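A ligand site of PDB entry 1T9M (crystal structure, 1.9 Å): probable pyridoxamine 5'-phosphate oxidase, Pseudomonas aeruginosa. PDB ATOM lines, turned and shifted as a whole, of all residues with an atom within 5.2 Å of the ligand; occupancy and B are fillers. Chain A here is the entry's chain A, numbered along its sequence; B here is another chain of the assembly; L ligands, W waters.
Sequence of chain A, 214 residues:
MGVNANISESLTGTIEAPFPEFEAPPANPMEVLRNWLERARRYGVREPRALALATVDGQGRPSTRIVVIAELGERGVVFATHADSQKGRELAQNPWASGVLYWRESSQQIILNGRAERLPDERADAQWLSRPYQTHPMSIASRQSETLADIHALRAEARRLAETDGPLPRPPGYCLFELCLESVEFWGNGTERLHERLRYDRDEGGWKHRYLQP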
ATOM      1  N   GLU A  47       8.146 -13.477  11.497  1.00  0.00           N
ATOM      2  CA  GLU A  47       9.082 -13.254  12.633  1.00  0.00           C
ATOM      3  C   GLU A  47       8.346 -12.736  13.895  1.00  0.00           C
ATOM      4  O   GLU A  47       8.591 -11.601  14.389  1.00  0.00           O
ATOM      5  CB  GLU A  47      10.202 -12.287  12.207  1.00  0.00           C
ATOM      6  CG  GLU A  47      11.059 -12.793  11.078  1.00  0.00           C
ATOM      7  CD  GLU A  47      12.179 -11.868  10.619  1.00  0.00           C
ATOM      8  OE1 GLU A  47      12.782 -11.195  11.456  1.00  0.00           O
ATOM      9  OE2 GLU A  47      12.416 -11.801   9.388  1.00  0.00           O
ATOM     10  N   ALA A  50      10.622 -11.543  17.080  1.00  0.00           N
ATOM     11  CA  ALA A  50      11.652 -10.462  16.949  1.00  0.00           C
ATOM     12  C   ALA A  50      11.266  -9.420  17.994  1.00  0.00           C
ATOM     13  O   ALA A  50      10.287  -8.653  17.813  1.00  0.00           O
ATOM     14  CB  ALA A  50      11.625  -9.869  15.564  1.00  0.00           C
ATOM     15  N   SER A  63      18.586   2.372  25.411  1.00  0.00           N
ATOM     16  CA  SER A  63      18.982   2.000  24.081  1.00  0.00           C
ATOM     17  C   SER A  63      18.086   0.793  23.604  1.00  0.00           C
ATOM     18  O   SER A  63      17.473   0.098  24.403  1.00  0.00           O
ATOM     19  CB  SER A  63      20.471   1.522  24.031  1.00  0.00           C
ATOM     20  OG  SER A  63      20.606   0.370  24.868  1.00  0.00           O
ATOM     21  N   THR A  64      17.942   0.641  22.305  1.00  0.00           N
ATOM     22  CA  THR A  64      17.077  -0.449  21.850  1.00  0.00           C
ATOM     23  C   THR A  64      17.755  -1.203  20.682  1.00  0.00           C
ATOM     24  O   THR A  64      18.702  -0.641  19.985  1.00  0.00           O
ATOM     25  CB  THR A  64      15.704   0.097  21.308  1.00  0.00           C
ATOM     26  OG1 THR A  64      16.036   1.132  20.416  1.00  0.00           O
ATOM     27  CG2 THR A  64      14.820   0.733  22.421  1.00  0.00           C
ATOM     28  N   ARG A  65      17.258  -2.447  20.435  1.00  0.00           N
ATOM     29  CA  ARG A  65      17.637  -3.201  19.217  1.00  0.00           C
ATOM     30  C   ARG A  65      16.737  -4.412  19.163  1.00  0.00           C
ATOM     31  O   ARG A  65      16.069  -4.749  20.164  1.00  0.00           O
ATOM     32  CB  ARG A  65      19.130  -3.685  19.272  1.00  0.00           C
ATOM     33  CG  ARG A  65      19.423  -4.748  20.305  1.00  0.00           C
ATOM     34  CD  ARG A  65      19.046  -4.343  21.838  1.00  0.00           C
ATOM     35  NE  ARG A  65      20.108  -3.435  22.267  1.00  0.00           N
ATOM     36  CZ  ARG A  65      20.096  -2.695  23.358  1.00  0.00           C
ATOM     37  NH1 ARG A  65      19.057  -2.766  24.144  1.00  0.00           N
ATOM     38  NH2 ARG A  65      21.195  -1.974  23.712  1.00  0.00           N
ATOM     39  N   ILE A  66      16.767  -5.143  18.038  1.00  0.00           N
ATOM     40  CA  ILE A  66      16.039  -6.398  17.991  1.00  0.00           C
ATOM     41  C   ILE A  66      16.910  -7.585  18.494  1.00  0.00           C
ATOM     42  O   ILE A  66      18.087  -7.685  18.162  1.00  0.00           O
ATOM     43  CB  ILE A  66      15.608  -6.691  16.567  1.00  0.00           C
ATOM     44  CG1 ILE A  66      14.686  -5.534  16.043  1.00  0.00           C
ATOM     45  CG2 ILE A  66      14.857  -8.081  16.591  1.00  0.00           C
ATOM     46  CD1 ILE A  66      13.227  -5.535  16.757  1.00  0.00           C
ATOM     47  N   VAL A  67      16.266  -8.462  19.267  1.00  0.00           N
ATOM     48  CA  VAL A  67      16.851  -9.767  19.616  1.00  0.00           C
ATOM     49  C   VAL A  67      15.712 -10.733  19.467  1.00  0.00           C
ATOM     50  O   VAL A  67      14.534 -10.317  19.522  1.00  0.00           O
ATOM     51  CB  VAL A  67      17.393  -9.804  21.082  1.00  0.00           C
ATOM     52  CG1 VAL A  67      18.450  -8.730  21.274  1.00  0.00           C
ATOM     53  CG2 VAL A  67      16.221  -9.733  22.147  1.00  0.00           C
ATOM     54  N   VAL A  68      16.033 -11.997  19.254  1.00  0.00           N
ATOM     55  CA  VAL A  68      15.003 -13.011  19.057  1.00  0.00           C
ATOM     56  C   VAL A  68      14.754 -13.750  20.389  1.00  0.00           C
ATOM     57  O   VAL A  68      15.707 -14.018  21.143  1.00  0.00           O
ATOM     58  CB  VAL A  68      15.465 -14.062  17.979  1.00  0.00           C
ATOM     59  CG1 VAL A  68      14.468 -15.222  17.831  1.00  0.00           C
ATOM     60  CG2 VAL A  68      15.547 -13.433  16.695  1.00  0.00           C
ATOM     61  N   ALA A  80      19.399 -14.844  23.587  1.00  0.00           N
ATOM     62  CA  ALA A  80      20.871 -15.050  23.563  1.00  0.00           C
ATOM     63  C   ALA A  80      21.554 -13.753  23.101  1.00  0.00           C
ATOM     64  O   ALA A  80      21.052 -13.077  22.197  1.00  0.00           O
ATOM     65  CB  ALA A  80      21.238 -16.188  22.576  1.00  0.00           C
ATOM     66  N   THR A  81      22.702 -13.392  23.700  1.00  0.00           N
ATOM     67  CA  THR A  81      23.440 -12.290  23.171  1.00  0.00           C
ATOM     68  C   THR A  81      24.864 -12.383  23.739  1.00  0.00           C
ATOM     69  O   THR A  81      25.254 -13.423  24.240  1.00  0.00           O
ATOM     70  CB  THR A  81      22.763 -10.907  23.578  1.00  0.00           C
ATOM     71  OG1 THR A  81      23.415  -9.849  22.867  1.00  0.00           O
ATOM     72  CG2 THR A  81      22.946 -10.570  25.139  1.00  0.00           C
ATOM     73  N   HIS A  82      25.648 -11.334  23.566  1.00  0.00           N
ATOM     74  CA  HIS A  82      27.000 -11.284  24.098  1.00  0.00           C
ATOM     75  C   HIS A  82      27.052 -10.397  25.318  1.00  0.00           C
ATOM     76  O   HIS A  82      26.585  -9.257  25.298  1.00  0.00           O
ATOM     77  CB  HIS A  82      28.024 -10.844  23.030  1.00  0.00           C
ATOM     78  CG  HIS A  82      28.052 -11.787  21.872  1.00  0.00           C
ATOM     79  ND1 HIS A  82      28.863 -12.932  21.848  1.00  0.00           N
ATOM     80  CD2 HIS A  82      27.274 -11.844  20.757  1.00  0.00           C
ATOM     81  CE1 HIS A  82      28.618 -13.597  20.725  1.00  0.00           C
ATOM     82  NE2 HIS A  82      27.634 -12.971  20.057  1.00  0.00           N
ATOM     83  N   SER A  85      28.486  -6.898  24.784  1.00  0.00           N
ATOM     84  CA  SER A  85      27.751  -5.999  23.864  1.00  0.00           C
ATOM     85  C   SER A  85      27.251  -4.798  24.684  1.00  0.00           C
ATOM     86  O   SER A  85      27.295  -4.791  25.964  1.00  0.00           O
ATOM     87  CB  SER A  85      26.524  -6.697  23.220  1.00  0.00           C
ATOM     88  OG  SER A  85      25.623  -7.197  24.174  1.00  0.00           O
ATOM     89  N   GLN A  86      26.714  -3.774  23.988  1.00  0.00           N
ATOM     90  CA  GLN A  86      26.125  -2.651  24.754  1.00  0.00           C
ATOM     91  C   GLN A  86      24.987  -3.124  25.687  1.00  0.00           C
ATOM     92  O   GLN A  86      24.882  -2.736  26.872  1.00  0.00           O
ATOM     93  CB  GLN A  86      25.555  -1.567  23.781  1.00  0.00           C
ATOM     94  CG  GLN A  86      24.951  -0.338  24.565  1.00  0.00           C
ATOM     95  CD  GLN A  86      24.687   0.900  23.696  1.00  0.00           C
ATOM     96  OE1 GLN A  86      25.196   1.014  22.557  1.00  0.00           O
ATOM     97  NE2 GLN A  86      24.006   1.871  24.273  1.00  0.00           N
ATOM     98  N   LYS A  87      24.098  -3.939  25.140  1.00  0.00           N
ATOM     99  CA  LYS A  87      22.980  -4.401  25.948  1.00  0.00           C
ATOM    100  C   LYS A  87      23.412  -5.208  27.105  1.00  0.00           C
ATOM    101  O   LYS A  87      22.773  -5.117  28.171  1.00  0.00           O
ATOM    102  CB  LYS A  87      21.903  -5.179  25.176  1.00  0.00           C
ATOM    103  CG  LYS A  87      22.232  -6.719  24.954  1.00  0.00           C
ATOM    104  CD  LYS A  87      21.252  -7.306  23.842  1.00  0.00           C
ATOM    105  CE  LYS A  87      21.688  -6.815  22.347  1.00  0.00           C
ATOM    106  NZ  LYS A  87      23.165  -7.058  22.133  1.00  0.00           N
ATOM    107  N   GLY A  88      24.437  -6.034  26.902  1.00  0.00           N
ATOM    108  CA  GLY A  88      24.895  -6.842  28.004  1.00  0.00           C
ATOM    109  C   GLY A  88      25.606  -5.975  29.060  1.00  0.00           C
ATOM    110  O   GLY A  88      25.407  -6.210  30.257  1.00  0.00           O
ATOM    111  N   GLN A 144      31.030  -8.358  19.602  1.00  0.00           N
ATOM    112  CA  GLN A 144      29.787  -7.624  19.301  1.00  0.00           C
ATOM    113  C   GLN A 144      29.782  -6.196  19.902  1.00  0.00           C
ATOM    114  O   GLN A 144      29.976  -6.006  21.109  1.00  0.00           O
ATOM    115  CB  GLN A 144      28.604  -8.493  19.776  1.00  0.00           C
ATOM    116  CG  GLN A 144      27.198  -7.825  19.547  1.00  0.00           C
ATOM    117  CD  GLN A 144      26.055  -8.744  19.904  1.00  0.00           C
ATOM    118  OE1 GLN A 144      25.421  -9.423  19.015  1.00  0.00           O
ATOM    119  NE2 GLN A 144      25.769  -8.800  21.125  1.00  0.00           N
ATOM    120  N   SER A 145      29.529  -5.231  19.037  1.00  0.00           N
ATOM    121  CA  SER A 145      29.326  -3.822  19.348  1.00  0.00           C
ATOM    122  C   SER A 145      30.610  -3.022  19.690  1.00  0.00           C
ATOM    123  O   SER A 145      30.552  -1.841  19.937  1.00  0.00           O
ATOM    124  CB  SER A 145      28.255  -3.618  20.429  1.00  0.00           C
ATOM    125  OG  SER A 145      27.107  -4.429  20.165  1.00  0.00           O
ATOM    126  N   LEU B  11      16.356 -14.924   9.775  1.00  0.00           N
ATOM    127  CA  LEU B  11      15.609 -13.771   9.165  1.00  0.00           C
ATOM    128  C   LEU B  11      14.795 -14.193   7.939  1.00  0.00           C
ATOM    129  O   LEU B  11      15.137 -15.158   7.213  1.00  0.00           O
ATOM    130  CB  LEU B  11      16.557 -12.612   8.781  1.00  0.00           C
ATOM    131  CG  LEU B  11      17.299 -11.830   9.878  1.00  0.00           C
ATOM    132  CD1 LEU B  11      18.787 -12.055   9.731  1.00  0.00           C
ATOM    133  CD2 LEU B  11      17.022 -10.320   9.796  1.00  0.00           C
ATOM    134  N   TYR B 102      12.258  -1.833  12.683  1.00  0.00           N
ATOM    135  CA  TYR B 102      12.756  -3.087  12.115  1.00  0.00           C
ATOM    136  C   TYR B 102      11.875  -3.437  10.872  1.00  0.00           C
ATOM    137  O   TYR B 102      10.633  -3.540  10.958  1.00  0.00           O
ATOM    138  CB  TYR B 102      12.699  -4.233  13.142  1.00  0.00           C
ATOM    139  CG  TYR B 102      13.047  -5.603  12.502  1.00  0.00           C
ATOM    140  CD1 TYR B 102      14.070  -5.687  11.530  1.00  0.00           C
ATOM    141  CD2 TYR B 102      12.362  -6.766  12.847  1.00  0.00           C
ATOM    142  CE1 TYR B 102      14.413  -6.887  10.941  1.00  0.00           C
ATOM    143  CE2 TYR B 102      12.672  -7.995  12.233  1.00  0.00           C
ATOM    144  CZ  TYR B 102      13.686  -8.019  11.284  1.00  0.00           C
ATOM    145  OH  TYR B 102      13.967  -9.200  10.714  1.00  0.00           O
ATOM    146  N   GLN B 109      17.484  -2.640  10.250  1.00  0.00           N
ATOM    147  CA  GLN B 109      17.024  -2.042  11.456  1.00  0.00           C
ATOM    148  C   GLN B 109      17.584  -0.610  11.599  1.00  0.00           C
ATOM    149  O   GLN B 109      18.689  -0.337  11.140  1.00  0.00           O
ATOM    150  CB  GLN B 109      17.388  -3.054  12.538  1.00  0.00           C
ATOM    151  CG  GLN B 109      17.993  -2.579  13.671  1.00  0.00           C
ATOM    152  CD  GLN B 109      18.341  -3.763  14.632  1.00  0.00           C
ATOM    153  OE1 GLN B 109      19.355  -4.486  14.485  1.00  0.00           O
ATOM    154  NE2 GLN B 109      17.550  -3.879  15.615  1.00  0.00           N
ATOM    155  N   GLU B 185      22.007   4.214  14.823  1.00  0.00           N
ATOM    156  CA  GLU B 185      22.618   3.117  14.120  1.00  0.00           C
ATOM    157  C   GLU B 185      21.744   2.676  12.997  1.00  0.00           C
ATOM    158  O   GLU B 185      20.540   2.453  13.198  1.00  0.00           O
ATOM    159  CB  GLU B 185      22.809   1.909  15.053  1.00  0.00           C
ATOM    160  CG  GLU B 185      23.507   0.793  14.275  1.00  0.00           C
ATOM    161  CD  GLU B 185      23.814  -0.427  15.126  1.00  0.00           C
ATOM    162  OE1 GLU B 185      24.051  -0.264  16.348  1.00  0.00           O
ATOM    163  OE2 GLU B 185      23.744  -1.570  14.593  1.00  0.00           O
ATOM    164  N   TRP B 187      21.516  -0.582  10.592  1.00  0.00           N
ATOM    165  CA  TRP B 187      21.933  -1.968  10.604  1.00  0.00           C
ATOM    166  C   TRP B 187      21.328  -2.653   9.349  1.00  0.00           C
ATOM    167  O   TRP B 187      20.122  -2.543   9.047  1.00  0.00           O
ATOM    168  CB  TRP B 187      21.385  -2.619  11.863  1.00  0.00           C
ATOM    169  CG  TRP B 187      21.669  -4.062  12.104  1.00  0.00           C
ATOM    170  CD1 TRP B 187      22.522  -4.525  13.103  1.00  0.00           C
ATOM    171  CD2 TRP B 187      21.070  -5.247  11.508  1.00  0.00           C
ATOM    172  NE1 TRP B 187      22.526  -5.892  13.093  1.00  0.00           N
ATOM    173  CE2 TRP B 187      21.673  -6.370  12.132  1.00  0.00           C
ATOM    174  CE3 TRP B 187      20.136  -5.480  10.464  1.00  0.00           C
ATOM    175  CZ2 TRP B 187      21.364  -7.687  11.778  1.00  0.00           C
ATOM    176  CZ3 TRP B 187      19.824  -6.772  10.126  1.00  0.00           C
ATOM    177  CH2 TRP B 187      20.443  -7.880  10.773  1.00  0.00           C
ATOM    178  N   ARG B 197      26.931  -2.328  10.321  1.00  0.00           N
ATOM    179  CA  ARG B 197      26.487  -1.490  11.423  1.00  0.00           C
ATOM    180  C   ARG B 197      27.208  -0.186  11.317  1.00  0.00           C
ATOM    181  O   ARG B 197      28.421  -0.107  11.567  1.00  0.00           O
ATOM    182  CB  ARG B 197      26.824  -2.134  12.803  1.00  0.00           C
ATOM    183  CG  ARG B 197      26.253  -3.586  12.926  1.00  0.00           C
ATOM    184  CD  ARG B 197      26.399  -4.102  14.368  1.00  0.00           C
ATOM    185  NE  ARG B 197      25.783  -3.212  15.349  1.00  0.00           N
ATOM    186  CZ  ARG B 197      25.921  -3.389  16.619  1.00  0.00           C
ATOM    187  NH1 ARG B 197      26.632  -4.483  17.040  1.00  0.00           N
ATOM    188  NH2 ARG B 197      25.331  -2.550  17.462  1.00  0.00           N
ATOM    189  N   PRO B 214      29.368  -7.022  14.435  1.00  0.00           N
ATOM    190  CA  PRO B 214      27.995  -7.531  14.547  1.00  0.00           C
ATOM    191  C   PRO B 214      27.721  -8.452  15.740  1.00  0.00           C
ATOM    192  O   PRO B 214      26.528  -8.605  16.092  1.00  0.00           O
ATOM    193  CB  PRO B 214      27.838  -8.368  13.264  1.00  0.00           C
ATOM    194  CG  PRO B 214      29.229  -8.825  12.928  1.00  0.00           C
ATOM    195  CD  PRO B 214      30.086  -7.571  13.236  1.00  0.00           C
ATOM    196  OXT PRO B 214      28.682  -9.086  16.222  1.00  0.00           O
HETATM  197  N1  LIG L   1      21.687  -9.827  18.508  1.00  0.00           N
HETATM  198  C1  LIG L   1      21.857 -10.715  19.557  1.00  0.00           C
HETATM  199  O1  LIG L   1      22.792 -10.549  20.308  1.00  0.00           O
HETATM  200  N2  LIG L   1      20.957 -11.696  19.849  1.00  0.00           N
HETATM  201  C2  LIG L   1      19.905 -11.907  18.980  1.00  0.00           C
HETATM  202  O2  LIG L   1      19.022 -12.681  19.287  1.00  0.00           O
HETATM  203  C3  LIG L   1      19.707 -11.070  17.904  1.00  0.00           C
HETATM  204  N3  LIG L   1      18.657 -11.291  17.045  1.00  0.00           N
HETATM  205  C4  LIG L   1      18.447 -10.406  16.010  1.00  0.00           C
HETATM  206  C5  LIG L   1      17.325 -10.622  15.138  1.00  0.00           C
HETATM  207  C6  LIG L   1      17.113  -9.741  14.090  1.00  0.00           C
HETATM  208  C7  LIG L   1      15.682  -9.764  13.466  1.00  0.00           C
HETATM  209  C8  LIG L   1      17.998  -8.648  13.852  1.00  0.00           C
HETATM  210  C9  LIG L   1      17.631  -7.463  12.916  1.00  0.00           C
HETATM  211  C10 LIG L   1      19.117  -8.478  14.700  1.00  0.00           C
HETATM  212  C11 LIG L   1      19.315  -9.366  15.774  1.00  0.00           C
HETATM  213  N4  LIG L   1      20.445  -9.205  16.578  1.00  0.00           N
HETATM  214  C12 LIG L   1      20.588 -10.018  17.678  1.00  0.00           C
HETATM  215  C13 LIG L   1      21.358  -8.054  16.416  1.00  0.00           C
HETATM  216  C14 LIG L   1      20.974  -6.935  17.367  1.00  0.00           C
HETATM  217  O3  LIG L   1      19.930  -6.115  16.855  1.00  0.00           O
HETATM  218  C15 LIG L   1      22.196  -5.965  17.628  1.00  0.00           C
HETATM  219  O4  LIG L   1      22.752  -5.447  16.455  1.00  0.00           O
HETATM  220  C16 LIG L   1      23.312  -6.577  18.471  1.00  0.00           C
HETATM  221  O5  LIG L   1      22.831  -7.473  19.460  1.00  0.00           O
HETATM  222  C17 LIG L   1      24.103  -5.492  19.197  1.00  0.00           C
HETATM  223  O6  LIG L   1      23.198  -4.765  20.000  1.00  0.00           O
HETATM  224  P1  LIG L   1      23.833  -3.747  21.102  1.00  0.00           P
HETATM  225  O7  LIG L   1      22.761  -2.725  21.318  1.00  0.00           O
HETATM  226  O8  LIG L   1      24.175  -4.515  22.396  1.00  0.00           O
HETATM  227  O9  LIG L   1      24.965  -3.001  20.408  1.00  0.00           O
HETATM  228  O   HOH W   1      19.328 -14.429  16.053  1.00  0.00           O
HETATM  229  O   HOH W   2      24.591  -7.049  14.906  1.00  0.00           O
HETATM  230  O   HOH W   3      21.755 -13.641  16.828  1.00  0.00           O
HETATM  231  O   HOH W   4      21.942  -2.985  16.214  1.00  0.00           O
HETATM  232  O   HOH W   5      22.212  -1.815  18.538  1.00  0.00           O
HETATM  233  O   HOH W   6      21.409  -0.245  20.608  1.00  0.00           O
HETATM  234  O   HOH W   7      18.199 -14.821  21.019  1.00  0.00           O
HETATM  235  O   HOH W   8      25.636  -0.435  20.377  1.00  0.00           O
HETATM  236  O   HOH W   9      21.976 -11.483  14.689  1.00  0.00           O
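Glu 47 touches the ligand. CA of Val 67 touches N3 of the ligand (3.5 Å). Ser 85 touches the ligand (CB to O8, 3.3 Å). Leu 11 of chain B touches the ligand (CD2 to C7, 3.9 Å). Tyr 102 of chain B touches the ligand. Hydrophobic or aromatic side chains within 4 Å of the ligand: Ile 66, Val 67, Val 68, Leu 11 of chain B, Tyr 102 of chain B and Trp 187 of chain B. Within 4 Å of the ligand: Glu 47, Arg 65, Ile 66, Val 67, Val 68, Ala 80, Thr 81, Ser 85, Gln 86, Lys 87, Gln 144, Ser 145, Leu 11 of chain B, Tyr 102 of chain B, Gln 109 of chain B, Trp 187 of chain B and Arg 197 of chain B. The nearest printed residue that does not touch the ligand is His 82 (4.4 Å).
OG of Ser 145 lies within hydrogen-bond range of O9 of the ligand (2.6 Å). The side-chain hydroxyl (OG1) of Thr 81 lies within hydrogen-bond range of an oxygen (O1) of the ligand (2.7 Å). An oxygen (O8) of the ligand sits at hydrogen-bond distance from the backbone NH of Lys 87 (2.8 Å). NZ of Lys 87 lies within salt-bridge range of O8 of the ligand (2.7 Å). A nitrogen (N2) of the ligand lies within hydrogen-bond range of the backbone carbonyl oxygen of Ala 80. An oxygen (O3) of the ligand sits at hydrogen-bond distance from the backbone carbonyl oxygen (O) of Ile 66. The guanidinium group (NE) of Arg 65 is in salt-bridge range of an oxygen (O7) of the ligand, 2.9 Å away. An oxygen (O3) of the ligand sits at hydrogen-bond distance from the side-chain amide oxygen (OE1) of Gln 109 of chain B (2.9 Å). The guanidinium group (NH2) of Arg 197 of chain B lies within salt-bridge range of an oxygen (O9) of the ligand. An oxygen (O2) of the ligand sits at hydrogen-bond distance from the backbone NH of Val 68 (3.1 Å). N of Gln 86 is in hydrogen-bond range of O8 of the ligand (3.1 Å). OE1 of Gln 144 lies close to O1 of the ligand, 3.1 Å away. The indole nitrogen (NE1) of Trp 187 of chain B lies within hydrogen-bond range of an oxygen (O4) of the ligand, 3.4 Å away.
The side-chain amino group (NZ) of Lys 87 lies within hydrogen-bond range of the side-chain hydroxyl (OG1) of Thr 81 (2.9 Å). OG1 of Thr 81 is in hydrogen-bond range of NE2 of Gln 144 (3.1 Å). NE2 of Gln 109 of chain B lies close to N of Ile 66, at 2.8 Å. The guanidinium group of Arg 65 sits at hydrogen-bond distance from the side-chain hydroxyl of Ser 63 (2.7 Å). The backbone carbonyl oxygen (O) of Gln 109 of chain B is in hydrogen-bond range of the backbone NH (N) of Trp 187 of chain B. The side-chain amide nitrogen of Gln 144 sits close to the side-chain hydroxyl of Ser 85, 3.4 Å away. The side-chain hydroxyl (OH) of Tyr 102 of chain B is in hydrogen-bond range of the side-chain carboxylate (OE1) of Glu 47, 2.4 Å away. OG of Ser 85 sits at hydrogen-bond distance from O of His 82 (2.5 Å).
Water W4 lies within hydrogen-bond range of an oxygen (O4) of the ligand (2.6 Å), the side-chain carboxylate of Glu 185 of chain B (2.8 Å) and the side-chain amide oxygen of Gln 109 of chain B (3.5 Å). Water W8 bridges O9 of the ligand (2.7 Å) and OE1 of Gln 86 (2.7 Å). Water W7 lies within hydrogen-bond range of the backbone carbonyl oxygen (O) of Val 68 (2.6 Å), the backbone NH (N) of Ala 80 (2.8 Å) and an oxygen (O2) of the ligand (2.9 Å). Water W2 lies within hydrogen-bond range of the chain-end carboxylate (O) of Pro 214 of chain B (2.8 Å), an oxygen (O4) of the ligand (2.9 Å) and the indole nitrogen (NE1) of Trp 187 of chain B (3.0 Å). Water W6 bridges O of Thr 64 (2.8 Å) and O7 of the ligand (2.9 Å). Water W5 lies within hydrogen-bond range of O7 of the ligand (3.0 Å), OE1 of Glu 185 of chain B (3.3 Å) and NH2 of Arg 197 of chain B (3.4 Å).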
